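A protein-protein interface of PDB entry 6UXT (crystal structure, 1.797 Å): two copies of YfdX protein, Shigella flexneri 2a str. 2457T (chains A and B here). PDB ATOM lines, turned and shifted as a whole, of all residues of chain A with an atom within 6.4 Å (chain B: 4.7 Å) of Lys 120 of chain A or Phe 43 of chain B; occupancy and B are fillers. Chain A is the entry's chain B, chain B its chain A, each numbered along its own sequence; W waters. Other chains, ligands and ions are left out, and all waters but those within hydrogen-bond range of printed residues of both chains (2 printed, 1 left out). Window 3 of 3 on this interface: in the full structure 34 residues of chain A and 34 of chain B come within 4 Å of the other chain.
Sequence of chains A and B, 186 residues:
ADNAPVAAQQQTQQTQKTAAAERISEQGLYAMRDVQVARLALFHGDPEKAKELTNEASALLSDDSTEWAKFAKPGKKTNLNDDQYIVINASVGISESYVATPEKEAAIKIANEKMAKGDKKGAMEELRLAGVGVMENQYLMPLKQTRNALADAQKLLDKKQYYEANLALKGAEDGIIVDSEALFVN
No position is printed for both chains.
Of the 22 pairs that touch across the chains among the printed residues, none has its exchanged pair printed and touching as well.
The backbone carbonyl oxygen of Arg 39 of chain B sits at hydrogen-bond distance from the side-chain amide nitrogen of Asn 166 of chain B.
The backbone NH (N) of Leu 183 of chain A lies within hydrogen-bond range of the backbone carbonyl oxygen (O) of Val 134 of chain A, 3.1 Å away.
Among the printed residues, merely in contact across the chains: Ile 94 of chain A with Tyr 163 of chain B, Val 92 of chain A with Phe 43 of chain B, Lys 120 of chain A with His 44 of chain B, Phe 184 of chain A with Phe 43 of chain B, Met 124 of chain A with Phe 43 of chain B, Ile 94 of chain A with Arg 39 of chain B, Val 134 of chain A with Phe 43 of chain B, Ile 94 of chain A with Asn 166 of chain B, Val 92 of chain A with Leu 40 of chain B, Lys 120 of chain A with Gly 45 of chain B, Phe 184 of chain A with His 44 of chain B, Lys 120 of chain A with Phe 43 of chain B, Gly 118 of chain A with Gly 45 of chain B, Met 115 of chain A with Phe 43 of chain B, Leu 127 of chain A with Tyr 163 of chain B, Met 115 of chain A with Gly 45 of chain B, Ile 94 of chain A with Phe 43 of chain B, Leu 183 of chain A with Phe 43 of chain B, Met 115 of chain A with Tyr 163 of chain B and Leu 183 of chain A with His 44 of chain B.
Water W2 lies within hydrogen-bond range of O of Val 92 of chain A (2.8 Å) and NH1 of Arg 39 of chain B (3.3 Å).
Water W1 lies within hydrogen-bond range of the guanidinium group of Arg 39 of chain B (2.8 Å), the backbone NH of Ile 94 of chain A (2.9 Å) and the backbone carbonyl oxygen of Val 92 of chain A (3.5 Å).
Of chain B, only Phe 43 (3.7 Å), His 44 (3.5 Å) and Gly 45 (3.7 Å) come within 4 Å of Lys 120 of chain A.
Of the printed residues of chain A, Phe 43 of chain B touches Val 92, Ile 94, Met 115, Lys 120, Met 124, Val 134, Leu 183 and Phe 184.
Of the printed residues of chain A, His 44 of chain B touches Lys 120 (3.5 Å), Leu 183 (3.95 Å) and Phe 184 (3.7 Å).
Of the printed residues of chain B, Gly 118 of chain A touches Gly 45.
The nearest printed residue of chain B that does not touch Lys 120 of chain A is Leu 42 of chain B (6.1 Å).
The nearest residue of chain A that does not touch Phe 43 of chain B is Leu 127 of chain A (4.6 Å).
Of the 9 printed residues of chain B, 8 touch a printed residue of chain A.
Of the 19 printed residues of chain A, 10 touch a printed residue of chain B.
Hydrophobic or aromatic side chains of chain A within 4 Å of the printed part of chain B: Val 92, Ile 94, Met 115, Met 124, Leu 127, Val 134, Leu 183 and Phe 184.
Among the printed residues, 22 pairs touch across the chains.
NH1 of Arg 39 of chain B is in hydrogen-bond range of O of Val 92 of chain A.
The side-chain sulfur of Met 115 of chain A lies close to the backbone carbonyl oxygen of Leu 42 of chain B (3.3 Å).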
ATOM      1  N   VAL A  92      15.280  21.943 -15.776  1.00  0.00           N
ATOM      2  CA  VAL A  92      16.069  21.289 -16.817  1.00  0.00           C
ATOM      3  C   VAL A  92      16.107  19.787 -16.565  1.00  0.00           C
ATOM      4  O   VAL A  92      16.245  19.340 -15.421  1.00  0.00           O
ATOM      5  CB  VAL A  92      17.495  21.884 -16.871  1.00  0.00           C
ATOM      6  CG1 VAL A  92      18.441  20.968 -17.644  1.00  0.00           C
ATOM      7  CG2 VAL A  92      17.450  23.245 -17.508  1.00  0.00           C
ATOM      8  N   GLY A  93      15.986  19.006 -17.646  1.00  0.00           N
ATOM      9  CA  GLY A  93      16.111  17.558 -17.590  1.00  0.00           C
ATOM     10  C   GLY A  93      17.134  17.047 -18.584  1.00  0.00           C
ATOM     11  O   GLY A  93      17.038  17.351 -19.778  1.00  0.00           O
ATOM     12  N   ILE A  94      18.116  16.277 -18.121  1.00  0.00           N
ATOM     13  CA  ILE A  94      19.208  15.782 -18.965  1.00  0.00           C
ATOM     14  C   ILE A  94      19.063  14.274 -19.139  1.00  0.00           C
ATOM     15  O   ILE A  94      18.906  13.551 -18.149  1.00  0.00           O
ATOM     16  CB  ILE A  94      20.576  16.101 -18.337  1.00  0.00           C
ATOM     17  CG1 ILE A  94      20.770  17.610 -18.200  1.00  0.00           C
ATOM     18  CG2 ILE A  94      21.720  15.451 -19.161  1.00  0.00           C
ATOM     19  CD1 ILE A  94      21.967  17.982 -17.348  1.00  0.00           C
ATOM     20  N   LYS A 114      30.403  27.516 -25.765  1.00  0.00           N
ATOM     21  CA  LYS A 114      29.269  28.284 -26.267  1.00  0.00           C
ATOM     22  C   LYS A 114      28.408  28.822 -25.128  1.00  0.00           C
ATOM     23  O   LYS A 114      27.880  29.940 -25.220  1.00  0.00           O
ATOM     24  CB  LYS A 114      28.443  27.439 -27.232  1.00  0.00           C
ATOM     25  CG  LYS A 114      29.216  27.061 -28.513  1.00  0.00           C
ATOM     26  CD  LYS A 114      28.363  26.250 -29.468  1.00  0.00           C
ATOM     27  CE  LYS A 114      29.122  25.935 -30.776  1.00  0.00           C
ATOM     28  NZ  LYS A 114      29.279  27.138 -31.639  1.00  0.00           N
ATOM     29  N   MET A 115      28.242  28.046 -24.052  1.00  0.00           N
ATOM     30  CA  MET A 115      27.549  28.575 -22.880  1.00  0.00           C
ATOM     31  C   MET A 115      28.259  29.806 -22.332  1.00  0.00           C
ATOM     32  O   MET A 115      27.611  30.797 -21.971  1.00  0.00           O
ATOM     33  CB  MET A 115      27.432  27.502 -21.794  1.00  0.00           C
ATOM     34  CG  MET A 115      26.392  26.459 -22.097  1.00  0.00           C
ATOM     35  SD  MET A 115      26.209  25.244 -20.766  1.00  0.00           S
ATOM     36  CE  MET A 115      26.992  23.811 -21.497  1.00  0.00           C
ATOM     37  N   LYS A 117      30.040  31.943 -23.895  1.00  0.00           N
ATOM     38  CA  LYS A 117      29.784  33.060 -24.800  1.00  0.00           C
ATOM     39  C   LYS A 117      28.306  33.413 -24.900  1.00  0.00           C
ATOM     40  O   LYS A 117      27.946  34.293 -25.687  1.00  0.00           O
ATOM     41  CB  LYS A 117      30.318  32.752 -26.202  1.00  0.00           C
ATOM     42  CG  LYS A 117      31.820  32.590 -26.300  1.00  0.00           C
ATOM     43  CD  LYS A 117      32.203  32.041 -27.671  1.00  0.00           C
ATOM     44  CE  LYS A 117      33.554  32.571 -28.146  1.00  0.00           C
ATOM     45  NZ  LYS A 117      34.660  32.259 -27.196  1.00  0.00           N
ATOM     46  N   GLY A 118      27.441  32.748 -24.137  1.00  0.00           N
ATOM     47  CA  GLY A 118      26.015  33.007 -24.217  1.00  0.00           C
ATOM     48  C   GLY A 118      25.308  32.454 -25.440  1.00  0.00           C
ATOM     49  O   GLY A 118      24.130  32.777 -25.642  1.00  0.00           O
ATOM     50  N   ASP A 119      25.987  31.646 -26.269  1.00  0.00           N
ATOM     51  CA  ASP A 119      25.365  30.998 -27.431  1.00  0.00           C
ATOM     52  C   ASP A 119      24.593  29.770 -26.946  1.00  0.00           C
ATOM     53  O   ASP A 119      24.957  28.619 -27.195  1.00  0.00           O
ATOM     54  CB  ASP A 119      26.407  30.613 -28.472  1.00  0.00           C
ATOM     55  CG  ASP A 119      25.793  29.988 -29.737  1.00  0.00           C
ATOM     56  OD1 ASP A 119      24.545  29.980 -29.901  1.00  0.00           O
ATOM     57  OD2 ASP A 119      26.574  29.497 -30.583  1.00  0.00           O
ATOM     58  N   LYS A 120      23.498  30.050 -26.240  1.00  0.00           N
ATOM     59  CA  LYS A 120      22.749  28.994 -25.567  1.00  0.00           C
ATOM     60  C   LYS A 120      22.172  27.989 -26.555  1.00  0.00           C
ATOM     61  O   LYS A 120      22.091  26.790 -26.252  1.00  0.00           O
ATOM     62  CB  LYS A 120      21.631  29.609 -24.718  1.00  0.00           C
ATOM     63  CG  LYS A 120      20.666  30.478 -25.507  1.00  0.00           C
ATOM     64  CD  LYS A 120      19.809  31.343 -24.583  1.00  0.00           C
ATOM     65  CE  LYS A 120      18.867  32.226 -25.387  1.00  0.00           C
ATOM     66  NZ  LYS A 120      18.089  33.155 -24.524  1.00  0.00           N
ATOM     67  N   LYS A 121      21.746  28.448 -27.733  1.00  0.00           N
ATOM     68  CA  LYS A 121      21.129  27.514 -28.668  1.00  0.00           C
ATOM     69  C   LYS A 121      22.174  26.602 -29.294  1.00  0.00           C
ATOM     70  O   LYS A 121      21.965  25.389 -29.393  1.00  0.00           O
ATOM     71  CB  LYS A 121      20.340  28.270 -29.737  1.00  0.00           C
ATOM     72  CG  LYS A 121      19.300  29.214 -29.142  1.00  0.00           C
ATOM     73  CD  LYS A 121      18.221  29.595 -30.137  1.00  0.00           C
ATOM     74  CE  LYS A 121      17.246  30.589 -29.527  1.00  0.00           C
ATOM     75  NZ  LYS A 121      16.148  30.916 -30.476  1.00  0.00           N
ATOM     76  N   GLY A 122      23.314  27.163 -29.714  1.00  0.00           N
ATOM     77  CA  GLY A 122      24.399  26.318 -30.190  1.00  0.00           C
ATOM     78  C   GLY A 122      24.894  25.332 -29.146  1.00  0.00           C
ATOM     79  O   GLY A 122      25.311  24.221 -29.481  1.00  0.00           O
ATOM     80  N   ALA A 123      24.871  25.719 -27.871  1.00  0.00           N
ATOM     81  CA  ALA A 123      25.353  24.809 -26.837  1.00  0.00           C
ATOM     82  C   ALA A 123      24.449  23.593 -26.719  1.00  0.00           C
ATOM     83  O   ALA A 123      24.938  22.463 -26.584  1.00  0.00           O
ATOM     84  CB  ALA A 123      25.448  25.519 -25.486  1.00  0.00           C
ATOM     85  N   MET A 124      23.129  23.807 -26.736  1.00  0.00           N
ATOM     86  CA  MET A 124      22.217  22.675 -26.606  1.00  0.00           C
ATOM     87  C   MET A 124      22.246  21.819 -27.862  1.00  0.00           C
ATOM     88  O   MET A 124      22.125  20.596 -27.785  1.00  0.00           O
ATOM     89  CB  MET A 124      20.799  23.156 -26.300  1.00  0.00           C
ATOM     90  CG  MET A 124      20.657  23.912 -24.966  1.00  0.00           C
ATOM     91  SD  MET A 124      21.173  22.946 -23.517  1.00  0.00           S
ATOM     92  CE  MET A 124      22.832  23.585 -23.207  1.00  0.00           C
ATOM     93  N   GLU A 125      22.406  22.446 -29.033  1.00  0.00           N
ATOM     94  CA  GLU A 125      22.516  21.677 -30.269  1.00  0.00           C
ATOM     95  C   GLU A 125      23.766  20.807 -30.265  1.00  0.00           C
ATOM     96  O   GLU A 125      23.730  19.650 -30.707  1.00  0.00           O
ATOM     97  CB  GLU A 125      22.523  22.614 -31.478  1.00  0.00           C
ATOM     98  CG  GLU A 125      21.143  22.952 -32.015  1.00  0.00           C
ATOM     99  CD  GLU A 125      20.383  21.727 -32.503  1.00  0.00           C
ATOM    100  OE1 GLU A 125      19.240  21.524 -32.046  1.00  0.00           O
ATOM    101  OE2 GLU A 125      20.926  20.972 -33.343  1.00  0.00           O
ATOM    102  N   LEU A 127      25.261  19.458 -27.672  1.00  0.00           N
ATOM    103  CA  LEU A 127      24.996  18.297 -26.821  1.00  0.00           C
ATOM    104  C   LEU A 127      24.088  17.291 -27.523  1.00  0.00           C
ATOM    105  O   LEU A 127      24.345  16.077 -27.517  1.00  0.00           O
ATOM    106  CB  LEU A 127      24.363  18.762 -25.511  1.00  0.00           C
ATOM    107  CG  LEU A 127      25.243  19.638 -24.635  1.00  0.00           C
ATOM    108  CD1 LEU A 127      24.468  20.059 -23.377  1.00  0.00           C
ATOM    109  CD2 LEU A 127      26.514  18.906 -24.264  1.00  0.00           C
ATOM    110  N   VAL A 134      18.614  17.390 -23.864  1.00  0.00           N
ATOM    111  CA  VAL A 134      18.254  18.366 -22.836  1.00  0.00           C
ATOM    112  C   VAL A 134      16.825  18.826 -23.074  1.00  0.00           C
ATOM    113  O   VAL A 134      16.505  19.346 -24.152  1.00  0.00           O
ATOM    114  CB  VAL A 134      19.207  19.571 -22.813  1.00  0.00           C
ATOM    115  CG1 VAL A 134      18.692  20.601 -21.805  1.00  0.00           C
ATOM    116  CG2 VAL A 134      20.621  19.129 -22.442  1.00  0.00           C
ATOM    117  N   MET A 135      15.976  18.657 -22.062  1.00  0.00           N
ATOM    118  CA  MET A 135      14.597  19.122 -22.091  1.00  0.00           C
ATOM    119  C   MET A 135      14.428  20.294 -21.140  1.00  0.00           C
ATOM    120  O   MET A 135      15.084  20.366 -20.099  1.00  0.00           O
ATOM    121  CB  MET A 135      13.613  18.017 -21.671  1.00  0.00           C
ATOM    122  CG  MET A 135      13.711  16.736 -22.482  1.00  0.00           C
ATOM    123  SD  MET A 135      13.325  16.966 -24.222  1.00  0.00           S
ATOM    124  CE  MET A 135      11.544  17.107 -24.171  1.00  0.00           C
ATOM    125  N   LEU A 183      15.122  21.696 -25.549  1.00  0.00           N
ATOM    126  CA  LEU A 183      15.508  23.083 -25.322  1.00  0.00           C
ATOM    127  C   LEU A 183      16.224  23.652 -26.549  1.00  0.00           C
ATOM    128  O   LEU A 183      17.275  23.140 -26.953  1.00  0.00           O
ATOM    129  CB  LEU A 183      16.399  23.173 -24.085  1.00  0.00           C
ATOM    130  CG  LEU A 183      16.892  24.570 -23.685  1.00  0.00           C
ATOM    131  CD1 LEU A 183      15.729  25.543 -23.492  1.00  0.00           C
ATOM    132  CD2 LEU A 183      17.767  24.500 -22.433  1.00  0.00           C
ATOM    133  N   PHE A 184      15.665  24.727 -27.117  1.00  0.00           N
ATOM    134  CA  PHE A 184      16.249  25.404 -28.288  1.00  0.00           C
ATOM    135  C   PHE A 184      16.389  24.468 -29.490  1.00  0.00           C
ATOM    136  O   PHE A 184      17.338  24.588 -30.272  1.00  0.00           O
ATOM    137  CB  PHE A 184      17.615  26.022 -27.963  1.00  0.00           C
ATOM    138  CG  PHE A 184      17.590  26.959 -26.796  1.00  0.00           C
ATOM    139  CD1 PHE A 184      16.558  27.873 -26.646  1.00  0.00           C
ATOM    140  CD2 PHE A 184      18.585  26.910 -25.841  1.00  0.00           C
ATOM    141  CE1 PHE A 184      16.523  28.736 -25.561  1.00  0.00           C
ATOM    142  CE2 PHE A 184      18.559  27.761 -24.753  1.00  0.00           C
ATOM    143  CZ  PHE A 184      17.523  28.677 -24.610  1.00  0.00           C
ATOM    144  N   ARG B  39      20.597  25.560 -12.469  1.00  0.00           N
ATOM    145  CA  ARG B  39      20.722  24.595 -13.560  1.00  0.00           C
ATOM    146  C   ARG B  39      20.092  25.136 -14.834  1.00  0.00           C
ATOM    147  O   ARG B  39      20.618  24.937 -15.937  1.00  0.00           O
ATOM    148  CB  ARG B  39      20.074  23.261 -13.155  1.00  0.00           C
ATOM    149  CG  ARG B  39      20.729  22.573 -11.967  1.00  0.00           C
ATOM    150  CD  ARG B  39      20.166  21.119 -11.716  1.00  0.00           C
ATOM    151  NE  ARG B  39      20.380  20.279 -12.900  1.00  0.00           N
ATOM    152  CZ  ARG B  39      19.448  19.558 -13.512  1.00  0.00           C
ATOM    153  NH1 ARG B  39      18.210  19.503 -13.030  1.00  0.00           N
ATOM    154  NH2 ARG B  39      19.766  18.864 -14.607  1.00  0.00           N
ATOM    155  N   LEU B  40      18.964  25.823 -14.700  1.00  0.00           N
ATOM    156  CA  LEU B  40      18.332  26.434 -15.858  1.00  0.00           C
ATOM    157  C   LEU B  40      19.201  27.557 -16.417  1.00  0.00           C
ATOM    158  O   LEU B  40      19.338  27.699 -17.637  1.00  0.00           O
ATOM    159  CB  LEU B  40      16.954  26.950 -15.451  1.00  0.00           C
ATOM    160  CG  LEU B  40      16.016  27.589 -16.474  1.00  0.00           C
ATOM    161  CD1 LEU B  40      15.477  26.553 -17.444  1.00  0.00           C
ATOM    162  CD2 LEU B  40      14.879  28.287 -15.728  1.00  0.00           C
ATOM    163  N   ALA B  41      19.828  28.339 -15.533  1.00  0.00           N
ATOM    164  CA  ALA B  41      20.620  29.489 -15.978  1.00  0.00           C
ATOM    165  C   ALA B  41      21.821  29.052 -16.800  1.00  0.00           C
ATOM    166  O   ALA B  41      22.155  29.693 -17.806  1.00  0.00           O
ATOM    167  CB  ALA B  41      21.075  30.318 -14.769  1.00  0.00           C
ATOM    168  N   LEU B  42      22.479  27.960 -16.394  1.00  0.00           N
ATOM    169  CA  LEU B  42      23.608  27.422 -17.146  1.00  0.00           C
ATOM    170  C   LEU B  42      23.238  27.128 -18.594  1.00  0.00           C
ATOM    171  O   LEU B  42      24.018  27.404 -19.509  1.00  0.00           O
ATOM    172  CB  LEU B  42      24.129  26.142 -16.488  1.00  0.00           C
ATOM    173  CG  LEU B  42      24.917  26.272 -15.185  1.00  0.00           C
ATOM    174  CD1 LEU B  42      25.063  24.905 -14.510  1.00  0.00           C
ATOM    175  CD2 LEU B  42      26.288  26.933 -15.439  1.00  0.00           C
ATOM    176  N   PHE B  43      22.059  26.564 -18.822  1.00  0.00           N
ATOM    177  CA  PHE B  43      21.704  26.137 -20.166  1.00  0.00           C
ATOM    178  C   PHE B  43      21.012  27.228 -20.958  1.00  0.00           C
ATOM    179  O   PHE B  43      20.740  27.040 -22.145  1.00  0.00           O
ATOM    180  CB  PHE B  43      20.817  24.891 -20.111  1.00  0.00           C
ATOM    181  CG  PHE B  43      21.567  23.631 -19.777  1.00  0.00           C
ATOM    182  CD1 PHE B  43      22.950  23.636 -19.669  1.00  0.00           C
ATOM    183  CD2 PHE B  43      20.893  22.441 -19.578  1.00  0.00           C
ATOM    184  CE1 PHE B  43      23.644  22.475 -19.366  1.00  0.00           C
ATOM    185  CE2 PHE B  43      21.582  21.270 -19.277  1.00  0.00           C
ATOM    186  CZ  PHE B  43      22.960  21.291 -19.170  1.00  0.00           C
ATOM    187  N   HIS B  44      20.694  28.342 -20.316  1.00  0.00           N
ATOM    188  CA  HIS B  44      20.272  29.546 -21.009  1.00  0.00           C
ATOM    189  C   HIS B  44      21.428  30.517 -21.209  1.00  0.00           C
ATOM    190  O   HIS B  44      21.200  31.710 -21.421  1.00  0.00           O
ATOM    191  CB  HIS B  44      19.113  30.195 -20.258  1.00  0.00           C
ATOM    192  CG  HIS B  44      17.821  29.462 -20.430  1.00  0.00           C
ATOM    193  ND1 HIS B  44      16.780  29.957 -21.186  1.00  0.00           N
ATOM    194  CD2 HIS B  44      17.422  28.247 -19.986  1.00  0.00           C
ATOM    195  CE1 HIS B  44      15.785  29.086 -21.180  1.00  0.00           C
ATOM    196  NE2 HIS B  44      16.150  28.040 -20.460  1.00  0.00           N
ATOM    197  N   GLY B  45      22.660  30.018 -21.164  1.00  0.00           N
ATOM    198  CA  GLY B  45      23.826  30.842 -21.443  1.00  0.00           C
ATOM    199  C   GLY B  45      24.066  31.945 -20.434  1.00  0.00           C
ATOM    200  O   GLY B  45      24.450  33.058 -20.814  1.00  0.00           O
ATOM    201  N   TYR B 163      28.426  22.094 -18.312  1.00  0.00           N
ATOM    202  CA  TYR B 163      27.577  20.907 -18.411  1.00  0.00           C
ATOM    203  C   TYR B 163      27.789  19.993 -17.217  1.00  0.00           C
ATOM    204  O   TYR B 163      26.825  19.509 -16.607  1.00  0.00           O
ATOM    205  CB  TYR B 163      27.850  20.145 -19.715  1.00  0.00           C
ATOM    206  CG  TYR B 163      27.090  18.829 -19.758  1.00  0.00           C
ATOM    207  CD1 TYR B 163      25.719  18.808 -19.996  1.00  0.00           C
ATOM    208  CD2 TYR B 163      27.738  17.620 -19.551  1.00  0.00           C
ATOM    209  CE1 TYR B 163      25.005  17.621 -20.015  1.00  0.00           C
ATOM    210  CE2 TYR B 163      27.036  16.422 -19.573  1.00  0.00           C
ATOM    211  CZ  TYR B 163      25.669  16.437 -19.811  1.00  0.00           C
ATOM    212  OH  TYR B 163      24.963  15.266 -19.822  1.00  0.00           O
ATOM    213  N   ASN B 166      26.141  21.217 -14.237  1.00  0.00           N
ATOM    214  CA  ASN B 166      24.704  21.001 -14.274  1.00  0.00           C
ATOM    215  C   ASN B 166      24.369  19.597 -13.774  1.00  0.00           C
ATOM    216  O   ASN B 166      23.427  19.413 -12.987  1.00  0.00           O
ATOM    217  CB  ASN B 166      24.184  21.244 -15.695  1.00  0.00           C
ATOM    218  CG  ASN B 166      22.721  21.665 -15.717  1.00  0.00           C
ATOM    219  OD1 ASN B 166      21.854  20.942 -15.228  1.00  0.00           O
ATOM    220  ND2 ASN B 166      22.449  22.848 -16.237  1.00  0.00           N
HETATM  221  O   HOH W   1      18.295  16.536 -15.257  1.00  0.00           O
HETATM  222  O   HOH W   2      14.921  19.035 -12.963  1.00  0.00           O
